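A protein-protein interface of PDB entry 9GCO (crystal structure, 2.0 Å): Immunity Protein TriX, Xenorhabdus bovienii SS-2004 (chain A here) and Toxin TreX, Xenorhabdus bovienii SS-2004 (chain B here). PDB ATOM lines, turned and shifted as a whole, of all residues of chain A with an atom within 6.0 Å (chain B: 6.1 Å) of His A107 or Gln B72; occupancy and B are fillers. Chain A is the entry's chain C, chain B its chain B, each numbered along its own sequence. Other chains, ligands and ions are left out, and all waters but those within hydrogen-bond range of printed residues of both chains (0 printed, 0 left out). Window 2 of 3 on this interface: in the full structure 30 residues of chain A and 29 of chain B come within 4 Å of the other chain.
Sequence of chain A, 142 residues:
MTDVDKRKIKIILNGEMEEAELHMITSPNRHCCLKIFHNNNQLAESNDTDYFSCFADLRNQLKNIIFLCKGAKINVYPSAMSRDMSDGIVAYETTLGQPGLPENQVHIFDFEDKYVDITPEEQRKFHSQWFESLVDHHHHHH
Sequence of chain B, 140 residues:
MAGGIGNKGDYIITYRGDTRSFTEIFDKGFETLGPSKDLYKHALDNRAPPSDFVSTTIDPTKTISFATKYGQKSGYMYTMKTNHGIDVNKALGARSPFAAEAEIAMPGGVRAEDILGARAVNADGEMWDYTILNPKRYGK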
ATOM      1  N   ARG A   7      -3.249   7.699 -15.627  1.00  0.00           N
ATOM      2  CA  ARG A   7      -4.613   7.339 -15.295  1.00  0.00           C
ATOM      3  C   ARG A   7      -5.156   6.420 -16.377  1.00  0.00           C
ATOM      4  O   ARG A   7      -4.974   6.675 -17.569  1.00  0.00           O
ATOM      5  CB  ARG A   7      -5.489   8.580 -15.149  1.00  0.00           C
ATOM      6  CG  ARG A   7      -6.891   8.203 -14.808  1.00  0.00           C
ATOM      7  CD  ARG A   7      -7.670   9.236 -14.018  1.00  0.00           C
ATOM      8  NE  ARG A   7      -8.987   8.691 -13.685  1.00  0.00           N
ATOM      9  CZ  ARG A   7      -9.860   9.252 -12.860  1.00  0.00           C
ATOM     10  NH1 ARG A   7      -9.559  10.334 -12.170  1.00  0.00           N
ATOM     11  NH2 ARG A   7     -11.066   8.712 -12.726  1.00  0.00           N
ATOM     12  N   MET A  24      -0.423  12.431 -18.151  1.00  0.00           N
ATOM     13  CA  MET A  24      -0.444  13.876 -17.957  1.00  0.00           C
ATOM     14  C   MET A  24       0.976  14.320 -17.619  1.00  0.00           C
ATOM     15  O   MET A  24       1.540  13.872 -16.617  1.00  0.00           O
ATOM     16  CB  MET A  24      -1.416  14.253 -16.839  1.00  0.00           C
ATOM     17  CG  MET A  24      -2.907  14.112 -17.193  1.00  0.00           C
ATOM     18  SD  MET A  24      -3.945  13.833 -15.730  1.00  0.00           S
ATOM     19  CE  MET A  24      -3.501  12.121 -15.382  1.00  0.00           C
ATOM     20  N   LYS A  70     -16.169  11.994 -17.934  1.00  0.00           N
ATOM     21  CA  LYS A  70     -16.992  13.166 -17.662  1.00  0.00           C
ATOM     22  C   LYS A  70     -16.585  14.322 -18.561  1.00  0.00           C
ATOM     23  O   LYS A  70     -17.427  15.139 -18.951  1.00  0.00           O
ATOM     24  CB  LYS A  70     -16.883  13.560 -16.180  1.00  0.00           C
ATOM     25  CG  LYS A  70     -17.508  12.625 -15.182  1.00  0.00           C
ATOM     26  CD  LYS A  70     -18.991  12.865 -15.038  1.00  0.00           C
ATOM     27  CE  LYS A  70     -19.601  11.941 -13.978  1.00  0.00           C
ATOM     28  NZ  LYS A  70     -21.085  12.062 -14.001  1.00  0.00           N
ATOM     29  N   GLY A  71     -15.279  14.450 -18.844  1.00  0.00           N
ATOM     30  CA  GLY A  71     -14.786  15.532 -19.696  1.00  0.00           C
ATOM     31  C   GLY A  71     -15.277  15.462 -21.127  1.00  0.00           C
ATOM     32  O   GLY A  71     -15.110  16.439 -21.876  1.00  0.00           O
ATOM     33  N   ILE A  89      -8.546  20.211 -14.916  1.00  0.00           N
ATOM     34  CA  ILE A  89      -8.858  18.864 -14.479  1.00  0.00           C
ATOM     35  C   ILE A  89     -10.222  18.820 -13.829  1.00  0.00           C
ATOM     36  O   ILE A  89     -10.878  17.777 -13.851  1.00  0.00           O
ATOM     37  CB  ILE A  89      -7.758  18.331 -13.543  1.00  0.00           C
ATOM     38  CG1 ILE A  89      -6.503  18.000 -14.356  1.00  0.00           C
ATOM     39  CG2 ILE A  89      -8.239  17.129 -12.751  1.00  0.00           C
ATOM     40  CD1 ILE A  89      -6.670  16.773 -15.259  1.00  0.00           C
ATOM     41  N   VAL A  90     -10.651  19.920 -13.202  1.00  0.00           N
ATOM     42  CA  VAL A  90     -11.958  20.004 -12.555  1.00  0.00           C
ATOM     43  C   VAL A  90     -12.877  20.847 -13.440  1.00  0.00           C
ATOM     44  O   VAL A  90     -12.518  21.971 -13.837  1.00  0.00           O
ATOM     45  CB  VAL A  90     -11.855  20.606 -11.142  1.00  0.00           C
ATOM     46  CG1 VAL A  90     -13.216  20.633 -10.459  1.00  0.00           C
ATOM     47  CG2 VAL A  90     -10.881  19.836 -10.291  1.00  0.00           C
ATOM     48  N   ALA A  91     -14.071  20.327 -13.696  1.00  0.00           N
ATOM     49  CA  ALA A  91     -15.070  20.945 -14.554  1.00  0.00           C
ATOM     50  C   ALA A  91     -16.417  20.807 -13.863  1.00  0.00           C
ATOM     51  O   ALA A  91     -16.520  20.242 -12.757  1.00  0.00           O
ATOM     52  CB  ALA A  91     -15.080  20.294 -15.938  1.00  0.00           C
ATOM     53  N   GLN A 105     -19.313  19.900  -9.424  1.00  0.00           N
ATOM     54  CA  GLN A 105     -17.932  19.745  -9.884  1.00  0.00           C
ATOM     55  C   GLN A 105     -17.629  18.272 -10.136  1.00  0.00           C
ATOM     56  O   GLN A 105     -18.143  17.402  -9.451  1.00  0.00           O
ATOM     57  CB  GLN A 105     -16.927  20.296  -8.865  1.00  0.00           C
ATOM     58  CG  GLN A 105     -16.917  21.809  -8.775  1.00  0.00           C
ATOM     59  CD  GLN A 105     -15.921  22.340  -7.765  1.00  0.00           C
ATOM     60  OE1 GLN A 105     -15.157  21.591  -7.132  1.00  0.00           O
ATOM     61  NE2 GLN A 105     -15.946  23.659  -7.576  1.00  0.00           N
ATOM     62  N   VAL A 106     -16.799  18.000 -11.145  1.00  0.00           N
ATOM     63  CA  VAL A 106     -16.375  16.647 -11.490  1.00  0.00           C
ATOM     64  C   VAL A 106     -14.920  16.693 -11.956  1.00  0.00           C
ATOM     65  O   VAL A 106     -14.443  17.708 -12.462  1.00  0.00           O
ATOM     66  CB  VAL A 106     -17.223  16.027 -12.626  1.00  0.00           C
ATOM     67  CG1 VAL A 106     -18.716  15.899 -12.213  1.00  0.00           C
ATOM     68  CG2 VAL A 106     -17.034  16.825 -13.909  1.00  0.00           C
ATOM     69  N   HIS A 107     -14.238  15.553 -11.824  1.00  0.00           N
ATOM     70  CA  HIS A 107     -12.903  15.330 -12.376  1.00  0.00           C
ATOM     71  C   HIS A 107     -13.092  14.879 -13.820  1.00  0.00           C
ATOM     72  O   HIS A 107     -13.898  13.992 -14.079  1.00  0.00           O
ATOM     73  CB  HIS A 107     -12.173  14.270 -11.556  1.00  0.00           C
ATOM     74  CG  HIS A 107     -10.738  14.079 -11.939  1.00  0.00           C
ATOM     75  ND1 HIS A 107     -10.356  13.560 -13.155  1.00  0.00           N
ATOM     76  CD2 HIS A 107      -9.590  14.292 -11.245  1.00  0.00           C
ATOM     77  CE1 HIS A 107      -9.034  13.494 -13.215  1.00  0.00           C
ATOM     78  NE2 HIS A 107      -8.544  13.923 -12.063  1.00  0.00           N
ATOM     79  N   ILE A 108     -12.373  15.494 -14.760  1.00  0.00           N
ATOM     80  CA  ILE A 108     -12.749  15.244 -16.144  1.00  0.00           C
ATOM     81  C   ILE A 108     -12.508  13.796 -16.571  1.00  0.00           C
ATOM     82  O   ILE A 108     -13.074  13.355 -17.593  1.00  0.00           O
ATOM     83  CB  ILE A 108     -12.054  16.160 -17.180  1.00  0.00           C
ATOM     84  CG1 ILE A 108     -10.528  16.054 -17.090  1.00  0.00           C
ATOM     85  CG2 ILE A 108     -12.571  17.591 -17.037  1.00  0.00           C
ATOM     86  CD1 ILE A 108      -9.770  16.940 -18.152  1.00  0.00           C
ATOM     87  N   PHE A 109     -11.683  13.036 -15.850  1.00  0.00           N
ATOM     88  CA  PHE A 109     -11.416  11.652 -16.249  1.00  0.00           C
ATOM     89  C   PHE A 109     -12.155  10.642 -15.382  1.00  0.00           C
ATOM     90  O   PHE A 109     -11.865   9.453 -15.453  1.00  0.00           O
ATOM     91  CB  PHE A 109      -9.906  11.400 -16.253  1.00  0.00           C
ATOM     92  CG  PHE A 109      -9.162  12.279 -17.213  1.00  0.00           C
ATOM     93  CD1 PHE A 109      -9.631  12.466 -18.513  1.00  0.00           C
ATOM     94  CD2 PHE A 109      -8.026  12.960 -16.824  1.00  0.00           C
ATOM     95  CE1 PHE A 109      -8.960  13.268 -19.398  1.00  0.00           C
ATOM     96  CE2 PHE A 109      -7.367  13.784 -17.711  1.00  0.00           C
ATOM     97  CZ  PHE A 109      -7.834  13.936 -18.994  1.00  0.00           C
ATOM     98  N   ASP A 110     -13.108  11.093 -14.573  1.00  0.00           N
ATOM     99  CA  ASP A 110     -14.020  10.185 -13.893  1.00  0.00           C
ATOM    100  C   ASP A 110     -14.963   9.544 -14.913  1.00  0.00           C
ATOM    101  O   ASP A 110     -15.312  10.146 -15.933  1.00  0.00           O
ATOM    102  CB  ASP A 110     -14.790  10.941 -12.807  1.00  0.00           C
ATOM    103  CG  ASP A 110     -15.724  10.029 -12.005  1.00  0.00           C
ATOM    104  OD1 ASP A 110     -15.422   8.817 -11.882  1.00  0.00           O
ATOM    105  OD2 ASP A 110     -16.742  10.519 -11.474  1.00  0.00           O
ATOM    106  N   PHE A 111     -15.382   8.309 -14.623  1.00  0.00           N
ATOM    107  CA  PHE A 111     -16.163   7.514 -15.561  1.00  0.00           C
ATOM    108  C   PHE A 111     -17.483   8.177 -15.912  1.00  0.00           C
ATOM    109  O   PHE A 111     -18.120   8.807 -15.071  1.00  0.00           O
ATOM    110  CB  PHE A 111     -16.462   6.133 -14.967  1.00  0.00           C
ATOM    111  CG  PHE A 111     -17.276   5.252 -15.871  1.00  0.00           C
ATOM    112  CD1 PHE A 111     -16.667   4.581 -16.914  1.00  0.00           C
ATOM    113  CD2 PHE A 111     -18.650   5.120 -15.694  1.00  0.00           C
ATOM    114  CE1 PHE A 111     -17.400   3.769 -17.781  1.00  0.00           C
ATOM    115  CE2 PHE A 111     -19.400   4.324 -16.538  1.00  0.00           C
ATOM    116  CZ  PHE A 111     -18.777   3.632 -17.599  1.00  0.00           C
ATOM    117  N   THR B  68      -6.154  20.573  -5.345  1.00  0.00           N
ATOM    118  CA  THR B  68      -5.904  19.133  -5.231  1.00  0.00           C
ATOM    119  C   THR B  68      -6.376  18.327  -6.439  1.00  0.00           C
ATOM    120  O   THR B  68      -6.240  17.091  -6.432  1.00  0.00           O
ATOM    121  CB  THR B  68      -6.566  18.572  -3.954  1.00  0.00           C
ATOM    122  OG1 THR B  68      -7.996  18.650  -4.054  1.00  0.00           O
ATOM    123  CG2 THR B  68      -6.100  19.334  -2.713  1.00  0.00           C
ATOM    124  N   LYS B  69      -6.917  18.978  -7.481  1.00  0.00           N
ATOM    125  CA  LYS B  69      -7.453  18.265  -8.650  1.00  0.00           C
ATOM    126  C   LYS B  69      -8.447  17.189  -8.211  1.00  0.00           C
ATOM    127  O   LYS B  69      -8.357  16.015  -8.588  1.00  0.00           O
ATOM    128  CB  LYS B  69      -6.313  17.686  -9.486  1.00  0.00           C
ATOM    129  CG  LYS B  69      -5.345  18.801  -9.924  1.00  0.00           C
ATOM    130  CD  LYS B  69      -4.471  18.429 -11.102  1.00  0.00           C
ATOM    131  CE  LYS B  69      -3.619  19.658 -11.504  1.00  0.00           C
ATOM    132  NZ  LYS B  69      -3.283  19.564 -12.928  1.00  0.00           N
ATOM    133  N   TYR B  70      -9.414  17.624  -7.398  1.00  0.00           N
ATOM    134  CA  TYR B  70     -10.493  16.784  -6.879  1.00  0.00           C
ATOM    135  C   TYR B  70      -9.962  15.665  -5.966  1.00  0.00           C
ATOM    136  O   TYR B  70     -10.347  14.491  -6.078  1.00  0.00           O
ATOM    137  CB  TYR B  70     -11.343  16.214  -8.029  1.00  0.00           C
ATOM    138  CG  TYR B  70     -12.808  16.051  -7.652  1.00  0.00           C
ATOM    139  CD1 TYR B  70     -13.660  17.153  -7.565  1.00  0.00           C
ATOM    140  CD2 TYR B  70     -13.317  14.807  -7.325  1.00  0.00           C
ATOM    141  CE1 TYR B  70     -14.981  17.009  -7.161  1.00  0.00           C
ATOM    142  CE2 TYR B  70     -14.624  14.655  -6.934  1.00  0.00           C
ATOM    143  CZ  TYR B  70     -15.462  15.745  -6.866  1.00  0.00           C
ATOM    144  OH  TYR B  70     -16.788  15.539  -6.502  1.00  0.00           O
ATOM    145  N   GLY B  71      -9.111  16.050  -5.019  1.00  0.00           N
ATOM    146  CA  GLY B  71      -8.590  15.110  -4.033  1.00  0.00           C
ATOM    147  C   GLY B  71      -7.615  14.092  -4.587  1.00  0.00           C
ATOM    148  O   GLY B  71      -7.467  13.018  -4.015  1.00  0.00           O
ATOM    149  N   GLN B  72      -6.924  14.415  -5.683  1.00  0.00           N
ATOM    150  CA  GLN B  72      -5.995  13.490  -6.320  1.00  0.00           C
ATOM    151  C   GLN B  72      -4.528  13.882  -6.210  1.00  0.00           C
ATOM    152  O   GLN B  72      -3.676  12.992  -6.269  1.00  0.00           O
ATOM    153  CB  GLN B  72      -6.328  13.344  -7.811  1.00  0.00           C
ATOM    154  CG  GLN B  72      -7.779  13.003  -8.109  1.00  0.00           C
ATOM    155  CD  GLN B  72      -8.194  11.661  -7.545  1.00  0.00           C
ATOM    156  OE1 GLN B  72      -7.564  10.633  -7.823  1.00  0.00           O
ATOM    157  NE2 GLN B  72      -9.269  11.663  -6.753  1.00  0.00           N
ATOM    158  N   LYS B  73      -4.200  15.175  -6.087  1.00  0.00           N
ATOM    159  CA  LYS B  73      -2.803  15.622  -6.086  1.00  0.00           C
ATOM    160  C   LYS B  73      -2.618  16.670  -4.991  1.00  0.00           C
ATOM    161  O   LYS B  73      -3.583  17.267  -4.518  1.00  0.00           O
ATOM    162  CB  LYS B  73      -2.388  16.227  -7.433  1.00  0.00           C
ATOM    163  CG  LYS B  73      -2.707  15.376  -8.671  1.00  0.00           C
ATOM    164  CD  LYS B  73      -1.738  14.200  -8.898  1.00  0.00           C
ATOM    165  CE  LYS B  73      -2.335  13.182  -9.911  1.00  0.00           C
ATOM    166  NZ  LYS B  73      -1.590  11.880 -10.020  1.00  0.00           N
ATOM    167  N   SER B  74      -1.371  16.886  -4.575  1.00  0.00           N
ATOM    168  CA  SER B  74      -1.100  17.999  -3.684  1.00  0.00           C
ATOM    169  C   SER B  74      -0.965  19.293  -4.490  1.00  0.00           C
ATOM    170  O   SER B  74      -0.822  19.287  -5.720  1.00  0.00           O
ATOM    171  CB  SER B  74       0.167  17.740  -2.858  1.00  0.00           C
ATOM    172  OG  SER B  74       1.283  17.656  -3.720  1.00  0.00           O
ATOM    173  N   ALA B 123      -3.345  15.743  -1.068  1.00  0.00           N
ATOM    174  CA  ALA B 123      -4.496  15.278  -1.828  1.00  0.00           C
ATOM    175  C   ALA B 123      -5.699  15.006  -0.933  1.00  0.00           C
ATOM    176  O   ALA B 123      -6.832  15.010  -1.419  1.00  0.00           O
ATOM    177  CB  ALA B 123      -4.159  14.008  -2.607  1.00  0.00           C
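N of Phe A109 lies within hydrogen-bond range of ND1 of His A107 (3.0 Å). NE2 of Gln B72 is in hydrogen-bond range of O of Tyr B70 (3.1 Å). O of Ile A89 sits at hydrogen-bond distance from N of Ile A108, 2.9 Å away. The guanidinium group of Arg A7 sits close to a ring nitrogen (ND1) of His A107 (3.5 Å).
Among the printed residues, pairs that only touch across the chains: Ile A89 with Lys B69 (3.8 Å), Val A90 with Tyr B70 (3.9 Å), Gln A105 with Tyr B70 (3.7 Å), His A107 with Lys B69 (3.4 Å) and His A107 with Gln B72 (3.8 Å).
His A107 touches just these residues of chain B: Lys B69 and Gln B72. Gln B72 touches just one residue of chain A: His A107. Printed residues of chain B within 4 Å of Ile A89: Lys B69 (3.8 Å). Of the printed residues of chain A, Lys B69 touches Ile A89 (3.8 Å) and His A107 (3.4 Å). Of the printed residues of chain B, Gln A105 touches Tyr B70. Of the printed residues of chain B, Val A90 touches Tyr B70. The nearest printed residue of chain A that does not touch Lys B69 is Val A90 (4.1 Å).
Of the 8 printed residues of chain B, 3 touch a printed residue of chain A. Printed residues of chain B that touch a printed residue of chain A: Lys B69, Tyr B70 and Gln B72. Hydrophobic or aromatic side chains of chain B that line the printed part of chain A: Tyr B70. Hydrophobic or aromatic side chains of chain A that line the printed part of chain B: Ile A89, Val A90 and His A107. Among the printed residues, no Asp or Glu carboxylate lies within 4 Å of a Lys or Arg side-chain nitrogen of the other chain.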
